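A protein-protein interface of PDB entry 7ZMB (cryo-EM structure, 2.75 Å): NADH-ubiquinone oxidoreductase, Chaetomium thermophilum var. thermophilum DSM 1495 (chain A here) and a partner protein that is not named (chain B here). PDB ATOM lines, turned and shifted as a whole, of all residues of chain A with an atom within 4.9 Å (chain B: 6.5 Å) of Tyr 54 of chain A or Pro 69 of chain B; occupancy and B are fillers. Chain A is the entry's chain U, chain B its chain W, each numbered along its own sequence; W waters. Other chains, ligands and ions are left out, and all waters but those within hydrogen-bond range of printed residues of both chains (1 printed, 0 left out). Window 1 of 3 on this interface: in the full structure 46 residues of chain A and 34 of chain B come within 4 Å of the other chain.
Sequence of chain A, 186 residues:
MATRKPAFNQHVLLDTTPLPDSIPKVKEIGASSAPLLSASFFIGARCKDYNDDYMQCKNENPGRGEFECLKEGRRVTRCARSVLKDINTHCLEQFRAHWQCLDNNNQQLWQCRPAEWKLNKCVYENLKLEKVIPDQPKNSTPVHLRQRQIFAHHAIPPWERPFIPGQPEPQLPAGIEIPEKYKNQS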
ATOM      1  N   TYR A  50      -4.623 -20.180  21.771  1.00  0.00           N
ATOM      2  CA  TYR A  50      -3.551 -19.967  20.770  1.00  0.00           C
ATOM      3  C   TYR A  50      -4.072 -20.318  19.381  1.00  0.00           C
ATOM      4  O   TYR A  50      -3.845 -19.538  18.448  1.00  0.00           O
ATOM      5  CB  TYR A  50      -2.309 -20.729  21.227  1.00  0.00           C
ATOM      6  CG  TYR A  50      -1.904 -20.380  22.637  1.00  0.00           C
ATOM      7  CD1 TYR A  50      -2.386 -21.089  23.724  1.00  0.00           C
ATOM      8  CD2 TYR A  50      -1.080 -19.298  22.886  1.00  0.00           C
ATOM      9  CE1 TYR A  50      -2.036 -20.749  25.021  1.00  0.00           C
ATOM     10  CE2 TYR A  50      -0.716 -18.947  24.174  1.00  0.00           C
ATOM     11  CZ  TYR A  50      -1.195 -19.675  25.245  1.00  0.00           C
ATOM     12  OH  TYR A  50      -0.828 -19.328  26.511  1.00  0.00           O
ATOM     13  N   ASN A  51      -4.752 -21.459  19.249  1.00  0.00           N
ATOM     14  CA  ASN A  51      -5.374 -21.849  17.958  1.00  0.00           C
ATOM     15  C   ASN A  51      -6.358 -20.758  17.549  1.00  0.00           C
ATOM     16  O   ASN A  51      -6.316 -20.333  16.384  1.00  0.00           O
ATOM     17  CB  ASN A  51      -6.150 -23.159  18.082  1.00  0.00           C
ATOM     18  CG  ASN A  51      -5.265 -24.376  18.242  1.00  0.00           C
ATOM     19  OD1 ASN A  51      -4.042 -24.270  18.199  1.00  0.00           O
ATOM     20  ND2 ASN A  51      -5.871 -25.538  18.420  1.00  0.00           N
ATOM     21  N   ASP A  52      -7.187 -20.306  18.487  1.00  0.00           N
ATOM     22  CA  ASP A  52      -8.213 -19.266  18.199  1.00  0.00           C
ATOM     23  C   ASP A  52      -7.547 -17.930  17.876  1.00  0.00           C
ATOM     24  O   ASP A  52      -8.154 -17.148  17.130  1.00  0.00           O
ATOM     25  CB  ASP A  52      -9.250 -19.178  19.315  1.00  0.00           C
ATOM     26  CG  ASP A  52     -10.164 -20.387  19.405  1.00  0.00           C
ATOM     27  OD1 ASP A  52     -10.115 -21.232  18.493  1.00  0.00           O
ATOM     28  OD2 ASP A  52     -10.921 -20.469  20.390  1.00  0.00           O
ATOM     29  N   ASP A  53      -6.335 -17.697  18.371  1.00  0.00           N
ATOM     30  CA  ASP A  53      -5.662 -16.387  18.184  1.00  0.00           C
ATOM     31  C   ASP A  53      -5.041 -16.361  16.791  1.00  0.00           C
ATOM     32  O   ASP A  53      -5.139 -15.317  16.131  1.00  0.00           O
ATOM     33  CB  ASP A  53      -4.594 -16.144  19.245  1.00  0.00           C
ATOM     34  CG  ASP A  53      -4.203 -14.687  19.401  1.00  0.00           C
ATOM     35  OD1 ASP A  53      -5.088 -13.827  19.259  1.00  0.00           O
ATOM     36  OD2 ASP A  53      -3.013 -14.429  19.666  1.00  0.00           O
ATOM     37  N   TYR A  54      -4.407 -17.463  16.390  1.00  0.00           N
ATOM     38  CA  TYR A  54      -3.841 -17.586  15.019  1.00  0.00           C
ATOM     39  C   TYR A  54      -4.913 -17.270  13.976  1.00  0.00           C
ATOM     40  O   TYR A  54      -4.687 -16.395  13.140  1.00  0.00           O
ATOM     41  CB  TYR A  54      -3.133 -18.933  14.854  1.00  0.00           C
ATOM     42  CG  TYR A  54      -2.429 -19.122  13.537  1.00  0.00           C
ATOM     43  CD1 TYR A  54      -1.452 -18.234  13.129  1.00  0.00           C
ATOM     44  CD2 TYR A  54      -2.737 -20.181  12.703  1.00  0.00           C
ATOM     45  CE1 TYR A  54      -0.795 -18.391  11.925  1.00  0.00           C
ATOM     46  CE2 TYR A  54      -2.088 -20.354  11.492  1.00  0.00           C
ATOM     47  CZ  TYR A  54      -1.113 -19.454  11.105  1.00  0.00           C
ATOM     48  OH  TYR A  54      -0.459 -19.591   9.921  1.00  0.00           O
ATOM     49  N   MET A  55      -6.020 -18.001  14.002  1.00  0.00           N
ATOM     50  CA  MET A  55      -7.111 -17.868  13.005  1.00  0.00           C
ATOM     51  C   MET A  55      -7.748 -16.467  13.004  1.00  0.00           C
ATOM     52  O   MET A  55      -8.120 -16.024  11.917  1.00  0.00           O
ATOM     53  CB  MET A  55      -8.157 -18.958  13.257  1.00  0.00           C
ATOM     54  CG  MET A  55      -7.573 -20.349  13.328  1.00  0.00           C
ATOM     55  SD  MET A  55      -6.994 -20.929  11.726  1.00  0.00           S
ATOM     56  CE  MET A  55      -8.555 -21.151  10.877  1.00  0.00           C
ATOM     57  N   GLN A  56      -7.860 -15.810  14.164  1.00  0.00           N
ATOM     58  CA  GLN A  56      -8.453 -14.452  14.277  1.00  0.00           C
ATOM     59  C   GLN A  56      -7.447 -13.448  13.721  1.00  0.00           C
ATOM     60  O   GLN A  56      -7.890 -12.469  13.099  1.00  0.00           O
ATOM     61  CB  GLN A  56      -8.802 -14.102  15.715  1.00  0.00           C
ATOM     62  CG  GLN A  56     -10.176 -14.586  16.148  1.00  0.00           C
ATOM     63  CD  GLN A  56     -10.388 -14.387  17.627  1.00  0.00           C
ATOM     64  OE1 GLN A  56      -9.440 -14.275  18.398  1.00  0.00           O
ATOM     65  NE2 GLN A  56     -11.644 -14.345  18.033  1.00  0.00           N
ATOM     66  N   CYS A  57      -6.156 -13.718  13.874  1.00  0.00           N
ATOM     67  CA  CYS A  57      -5.123 -12.855  13.257  1.00  0.00           C
ATOM     68  C   CYS A  57      -5.226 -12.949  11.730  1.00  0.00           C
ATOM     69  O   CYS A  57      -5.164 -11.905  11.077  1.00  0.00           O
ATOM     70  CB  CYS A  57      -3.739 -13.295  13.723  1.00  0.00           C
ATOM     71  SG  CYS A  57      -2.385 -12.274  13.087  1.00  0.00           S
ATOM     72  N   LYS A  58      -5.358 -14.160  11.184  1.00  0.00           N
ATOM     73  CA  LYS A  58      -5.439 -14.343   9.712  1.00  0.00           C
ATOM     74  C   LYS A  58      -6.695 -13.649   9.177  1.00  0.00           C
ATOM     75  O   LYS A  58      -6.598 -13.019   8.122  1.00  0.00           O
ATOM     76  CB  LYS A  58      -5.271 -15.819   9.344  1.00  0.00           C
ATOM     77  CG  LYS A  58      -3.927 -16.422   9.722  1.00  0.00           C
ATOM     78  CD  LYS A  58      -3.707 -17.790   9.133  1.00  0.00           C
ATOM     79  CE  LYS A  58      -3.641 -17.778   7.622  1.00  0.00           C
ATOM     80  NZ  LYS A  58      -3.404 -19.138   7.087  1.00  0.00           N
ATOM     81  N   CYS A  69       1.097 -13.159  10.467  1.00  0.00           N
ATOM     82  CA  CYS A  69       0.690 -13.829  11.728  1.00  0.00           C
ATOM     83  C   CYS A  69       1.693 -14.922  12.114  1.00  0.00           C
ATOM     84  O   CYS A  69       1.275 -15.924  12.711  1.00  0.00           O
ATOM     85  CB  CYS A  69      -0.726 -14.376  11.608  1.00  0.00           C
ATOM     86  SG  CYS A  69      -1.950 -13.086  11.270  1.00  0.00           S
ATOM     87  N   GLU A  72       2.092 -16.016  15.993  1.00  0.00           N
ATOM     88  CA  GLU A  72       0.961 -16.839  16.487  1.00  0.00           C
ATOM     89  C   GLU A  72       1.163 -18.287  16.041  1.00  0.00           C
ATOM     90  O   GLU A  72       0.903 -19.183  16.843  1.00  0.00           O
ATOM     91  CB  GLU A  72      -0.351 -16.279  15.941  1.00  0.00           C
ATOM     92  CG  GLU A  72      -0.806 -14.984  16.585  1.00  0.00           C
ATOM     93  CD  GLU A  72       0.012 -13.746  16.257  1.00  0.00           C
ATOM     94  OE1 GLU A  72       0.688 -13.738  15.212  1.00  0.00           O
ATOM     95  OE2 GLU A  72      -0.024 -12.795  17.060  1.00  0.00           O
ATOM     96  N   GLY A  73       1.599 -18.495  14.799  1.00  0.00           N
ATOM     97  CA  GLY A  73       1.833 -19.853  14.280  1.00  0.00           C
ATOM     98  C   GLY A  73       2.921 -20.551  15.057  1.00  0.00           C
ATOM     99  O   GLY A  73       2.758 -21.743  15.354  1.00  0.00           O
ATOM    100  N   VAL A  76       1.344 -21.643  18.357  1.00  0.00           N
ATOM    101  CA  VAL A  76       0.498 -22.876  18.260  1.00  0.00           C
ATOM    102  C   VAL A  76       1.392 -24.111  18.173  1.00  0.00           C
ATOM    103  O   VAL A  76       1.070 -25.109  18.826  1.00  0.00           O
ATOM    104  CB  VAL A  76      -0.583 -22.837  17.153  1.00  0.00           C
ATOM    105  CG1 VAL A  76      -1.385 -21.550  17.192  1.00  0.00           C
ATOM    106  CG2 VAL A  76      -0.045 -23.092  15.758  1.00  0.00           C
ATOM    107  N   ARG B  64     -10.582 -32.640  13.776  1.00  0.00           N
ATOM    108  CA  ARG B  64      -9.839 -31.995  12.665  1.00  0.00           C
ATOM    109  C   ARG B  64      -9.624 -30.505  12.954  1.00  0.00           C
ATOM    110  O   ARG B  64      -8.534 -30.018  12.656  1.00  0.00           O
ATOM    111  CB  ARG B  64     -10.544 -32.242  11.329  1.00  0.00           C
ATOM    112  CG  ARG B  64     -10.456 -33.670  10.819  1.00  0.00           C
ATOM    113  CD  ARG B  64     -11.014 -33.768   9.419  1.00  0.00           C
ATOM    114  NE  ARG B  64     -10.796 -35.090   8.863  1.00  0.00           N
ATOM    115  CZ  ARG B  64     -11.121 -35.446   7.630  1.00  0.00           C
ATOM    116  NH1 ARG B  64     -10.880 -36.675   7.210  1.00  0.00           N
ATOM    117  NH2 ARG B  64     -11.675 -34.566   6.815  1.00  0.00           N
ATOM    118  N   ILE B  65     -10.607 -29.829  13.542  1.00  0.00           N
ATOM    119  CA  ILE B  65     -10.521 -28.366  13.816  1.00  0.00           C
ATOM    120  C   ILE B  65      -9.346 -28.079  14.759  1.00  0.00           C
ATOM    121  O   ILE B  65      -8.662 -27.077  14.529  1.00  0.00           O
ATOM    122  CB  ILE B  65     -11.873 -27.835  14.336  1.00  0.00           C
ATOM    123  CG1 ILE B  65     -12.808 -27.455  13.187  1.00  0.00           C
ATOM    124  CG2 ILE B  65     -11.690 -26.689  15.315  1.00  0.00           C
ATOM    125  CD1 ILE B  65     -14.260 -27.721  13.477  1.00  0.00           C
ATOM    126  N   HIS B  66      -9.081 -28.953  15.734  1.00  0.00           N
ATOM    127  CA  HIS B  66      -7.921 -28.774  16.650  1.00  0.00           C
ATOM    128  C   HIS B  66      -6.591 -28.884  15.883  1.00  0.00           C
ATOM    129  O   HIS B  66      -5.660 -28.136  16.211  1.00  0.00           O
ATOM    130  CB  HIS B  66      -8.020 -29.730  17.846  1.00  0.00           C
ATOM    131  CG  HIS B  66      -9.287 -29.633  18.627  1.00  0.00           C
ATOM    132  ND1 HIS B  66      -9.917 -28.431  18.878  1.00  0.00           N
ATOM    133  CD2 HIS B  66     -10.029 -30.583  19.236  1.00  0.00           C
ATOM    134  CE1 HIS B  66     -11.001 -28.647  19.592  1.00  0.00           C
ATOM    135  NE2 HIS B  66     -11.093 -29.957  19.826  1.00  0.00           N
ATOM    136  N   LEU B  67      -6.477 -29.831  14.963  1.00  0.00           N
ATOM    137  CA  LEU B  67      -5.235 -30.036  14.177  1.00  0.00           C
ATOM    138  C   LEU B  67      -5.022 -28.936  13.135  1.00  0.00           C
ATOM    139  O   LEU B  67      -3.863 -28.680  12.804  1.00  0.00           O
ATOM    140  CB  LEU B  67      -5.288 -31.439  13.573  1.00  0.00           C
ATOM    141  CG  LEU B  67      -5.390 -32.533  14.626  1.00  0.00           C
ATOM    142  CD1 LEU B  67      -5.843 -33.849  14.020  1.00  0.00           C
ATOM    143  CD2 LEU B  67      -4.077 -32.673  15.376  1.00  0.00           C
ATOM    144  N   ILE B  68      -6.093 -28.308  12.655  1.00  0.00           N
ATOM    145  CA  ILE B  68      -6.000 -27.306  11.556  1.00  0.00           C
ATOM    146  C   ILE B  68      -4.979 -26.205  11.853  1.00  0.00           C
ATOM    147  O   ILE B  68      -4.206 -25.912  10.931  1.00  0.00           O
ATOM    148  CB  ILE B  68      -7.398 -26.739  11.212  1.00  0.00           C
ATOM    149  CG1 ILE B  68      -8.181 -27.638  10.255  1.00  0.00           C
ATOM    150  CG2 ILE B  68      -7.318 -25.311  10.696  1.00  0.00           C
ATOM    151  CD1 ILE B  68      -9.562 -27.124   9.930  1.00  0.00           C
ATOM    152  N   PRO B  69      -4.887 -25.552  13.040  1.00  0.00           N
ATOM    153  CA  PRO B  69      -3.985 -24.398  13.179  1.00  0.00           C
ATOM    154  C   PRO B  69      -2.495 -24.725  13.226  1.00  0.00           C
ATOM    155  O   PRO B  69      -1.760 -23.964  12.695  1.00  0.00           O
ATOM    156  CB  PRO B  69      -4.433 -23.696  14.469  1.00  0.00           C
ATOM    157  CG  PRO B  69      -5.821 -24.249  14.697  1.00  0.00           C
ATOM    158  CD  PRO B  69      -5.721 -25.685  14.232  1.00  0.00           C
ATOM    159  N   LEU B  70      -2.113 -25.859  13.810  1.00  0.00           N
ATOM    160  CA  LEU B  70      -0.686 -26.277  13.833  1.00  0.00           C
ATOM    161  C   LEU B  70      -0.263 -26.810  12.466  1.00  0.00           C
ATOM    162  O   LEU B  70       0.921 -26.663  12.126  1.00  0.00           O
ATOM    163  CB  LEU B  70      -0.466 -27.289  14.961  1.00  0.00           C
ATOM    164  CG  LEU B  70      -1.338 -28.544  14.935  1.00  0.00           C
ATOM    165  CD1 LEU B  70      -0.557 -29.746  14.425  1.00  0.00           C
ATOM    166  CD2 LEU B  70      -1.900 -28.837  16.317  1.00  0.00           C
ATOM    167  N   LEU B  71      -1.202 -27.351  11.694  1.00  0.00           N
ATOM    168  CA  LEU B  71      -0.917 -27.826  10.310  1.00  0.00           C
ATOM    169  C   LEU B  71      -0.839 -26.618   9.374  1.00  0.00           C
ATOM    170  O   LEU B  71       0.089 -26.567   8.578  1.00  0.00           O
ATOM    171  CB  LEU B  71      -1.970 -28.851   9.894  1.00  0.00           C
ATOM    172  CG  LEU B  71      -1.889 -30.219  10.567  1.00  0.00           C
ATOM    173  CD1 LEU B  71      -3.172 -30.996  10.346  1.00  0.00           C
ATOM    174  CD2 LEU B  71      -0.702 -31.018  10.063  1.00  0.00           C
ATOM    175  N   GLN B  72      -1.814 -25.713   9.436  1.00  0.00           N
ATOM    176  CA  GLN B  72      -1.823 -24.492   8.590  1.00  0.00           C
ATOM    177  C   GLN B  72      -0.719 -23.528   9.026  1.00  0.00           C
ATOM    178  O   GLN B  72      -0.320 -22.712   8.211  1.00  0.00           O
ATOM    179  CB  GLN B  72      -3.212 -23.861   8.513  1.00  0.00           C
ATOM    180  CG  GLN B  72      -3.374 -22.835   7.401  1.00  0.00           C
ATOM    181  CD  GLN B  72      -3.220 -23.393   6.005  1.00  0.00           C
ATOM    182  OE1 GLN B  72      -3.235 -24.600   5.781  1.00  0.00           O
ATOM    183  NE2 GLN B  72      -3.080 -22.502   5.039  1.00  0.00           N
ATOM    184  N   ALA B  73      -0.179 -23.681  10.226  1.00  0.00           N
ATOM    185  CA  ALA B  73       0.944 -22.820  10.657  1.00  0.00           C
ATOM    186  C   ALA B  73       2.228 -23.324   9.996  1.00  0.00           C
ATOM    187  O   ALA B  73       3.022 -22.478   9.564  1.00  0.00           O
ATOM    188  CB  ALA B  73       1.067 -22.917  12.148  1.00  0.00           C
ATOM    189  N   GLU B  74       2.391 -24.638   9.889  1.00  0.00           N
ATOM    190  CA  GLU B  74       3.556 -25.255   9.211  1.00  0.00           C
ATOM    191  C   GLU B  74       3.498 -24.968   7.710  1.00  0.00           C
ATOM    192  O   GLU B  74       4.560 -24.699   7.124  1.00  0.00           O
ATOM    193  CB  GLU B  74       3.492 -26.759   9.458  1.00  0.00           C
ATOM    194  CG  GLU B  74       4.616 -27.544   8.818  1.00  0.00           C
ATOM    195  CD  GLU B  74       4.294 -29.016   8.651  1.00  0.00           C
ATOM    196  OE1 GLU B  74       4.960 -29.674   7.840  1.00  0.00           O
ATOM    197  OE2 GLU B  74       3.366 -29.493   9.326  1.00  0.00           O
ATOM    198  N   ASP B  76       2.081 -22.406   6.193  1.00  0.00           N
ATOM    199  CA  ASP B  76       2.363 -20.962   5.979  1.00  0.00           C
ATOM    200  C   ASP B  76       3.864 -20.695   6.065  1.00  0.00           C
ATOM    201  O   ASP B  76       4.358 -19.917   5.251  1.00  0.00           O
ATOM    202  CB  ASP B  76       1.592 -20.085   6.959  1.00  0.00           C
ATOM    203  CG  ASP B  76       0.087 -20.101   6.756  1.00  0.00           C
ATOM    204  OD1 ASP B  76      -0.399 -20.949   5.984  1.00  0.00           O
ATOM    205  OD2 ASP B  76      -0.585 -19.257   7.367  1.00  0.00           O
ATOM    206  N   ARG B  77       4.556 -21.343   7.002  1.00  0.00           N
ATOM    207  CA  ARG B  77       6.022 -21.164   7.116  1.00  0.00           C
ATOM    208  C   ARG B  77       6.674 -21.651   5.824  1.00  0.00           C
ATOM    209  O   ARG B  77       7.577 -20.966   5.342  1.00  0.00           O
ATOM    210  CB  ARG B  77       6.556 -21.827   8.387  1.00  0.00           C
ATOM    211  CG  ARG B  77       6.365 -20.998   9.646  1.00  0.00           C
ATOM    212  CD  ARG B  77       7.000 -21.704  10.824  1.00  0.00           C
ATOM    213  NE  ARG B  77       6.302 -22.928  11.174  1.00  0.00           N
ATOM    214  CZ  ARG B  77       5.417 -23.031  12.154  1.00  0.00           C
ATOM    215  NH1 ARG B  77       5.123 -21.979  12.897  1.00  0.00           N
ATOM    216  NH2 ARG B  77       4.835 -24.189  12.398  1.00  0.00           N
HETATM  217  O   HOH W   1      -9.046 -25.550  17.764  1.00  0.00           O
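Tyr 54 of chain A touches four residues of chain B. Of chain A, only Asn 51, Tyr 54 and Val 76 come within 4 Å of Pro 69 of chain B. Of the printed residues of chain A, Leu 70 of chain B touches Val 76 (3.8 Å). Of the printed residues of chain A, Arg 77 of chain B touches Gly 73 (3.4 Å). Of the printed residues of chain B, Gly 73 of chain A touches Ala 73 (3.8 Å) and Arg 77 (3.4 Å). Of the printed residues of chain B, Asn 51 of chain A touches His 66 and Pro 69. Of the printed residues of chain A, His 66 of chain B touches Asn 51. The nearest residue of chain A that does not touch Pro 69 of chain B is Met 55 of chain A (4.5 Å).
Among the printed residues, pairs that only touch across the chains: Tyr 54 of chain A with Gln 72 of chain B (3.6 Å), Asn 51 of chain A with Pro 69 of chain B (3.6 Å), Tyr 54 of chain A with Ala 73 of chain B (3.6 Å), Val 76 of chain A with Pro 69 of chain B (3.6 Å), Lys 58 of chain A with Gln 72 of chain B (3.7 Å), Val 76 of chain A with Leu 70 of chain B (3.8 Å), Val 76 of chain A with Ala 73 of chain B (3.8 Å), Gly 73 of chain A with Ala 73 of chain B (3.8 Å) and Tyr 54 of chain A with Pro 69 of chain B (3.8 Å).
Of the 13 printed residues of chain B, 7 touch a printed residue of chain A. Hydrophobic or aromatic side chains of chain B within 4 Å of the printed part of chain A: Pro 69 and Ala 73. Along chain B the printed residues that touch a printed residue of chain A span positions 66 to 77. Of the 13 printed residues of chain A, 5 touch a printed residue of chain B.
SG of Cys 57 of chain A forms a disulfide with SG of Cys 69 of chain A (2.0 Å). The backbone NH (N) of Lys 58 of chain A sits at hydrogen-bond distance from the side-chain sulfur (SG) of Cys 69 of chain A (3.6 Å). NE2 of Gln 72 of chain B sits at hydrogen-bond distance from OD1 of Asp 76 of chain B (3.2 Å).
Water W1 lies within hydrogen-bond range of ND1 of His 66 of chain B (3.2 Å) and ND2 of Asn 51 of chain A (3.2 Å).
OH of Tyr 54 of chain A sits at hydrogen-bond distance from OD2 of Asp 76 of chain B (2.6 Å). The guanidinium group (NH1) of Arg 77 of chain B sits close to the backbone carbonyl oxygen (O) of Gly 73 of chain A (3.4 Å). The side-chain amide nitrogen (ND2) of Asn 51 of chain A sits at hydrogen-bond distance from the backbone carbonyl oxygen (O) of His 66 of chain B (3.4 Å). NZ of Lys 58 of chain A lies within salt-bridge range of OD2 of Asp 76 of chain B.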
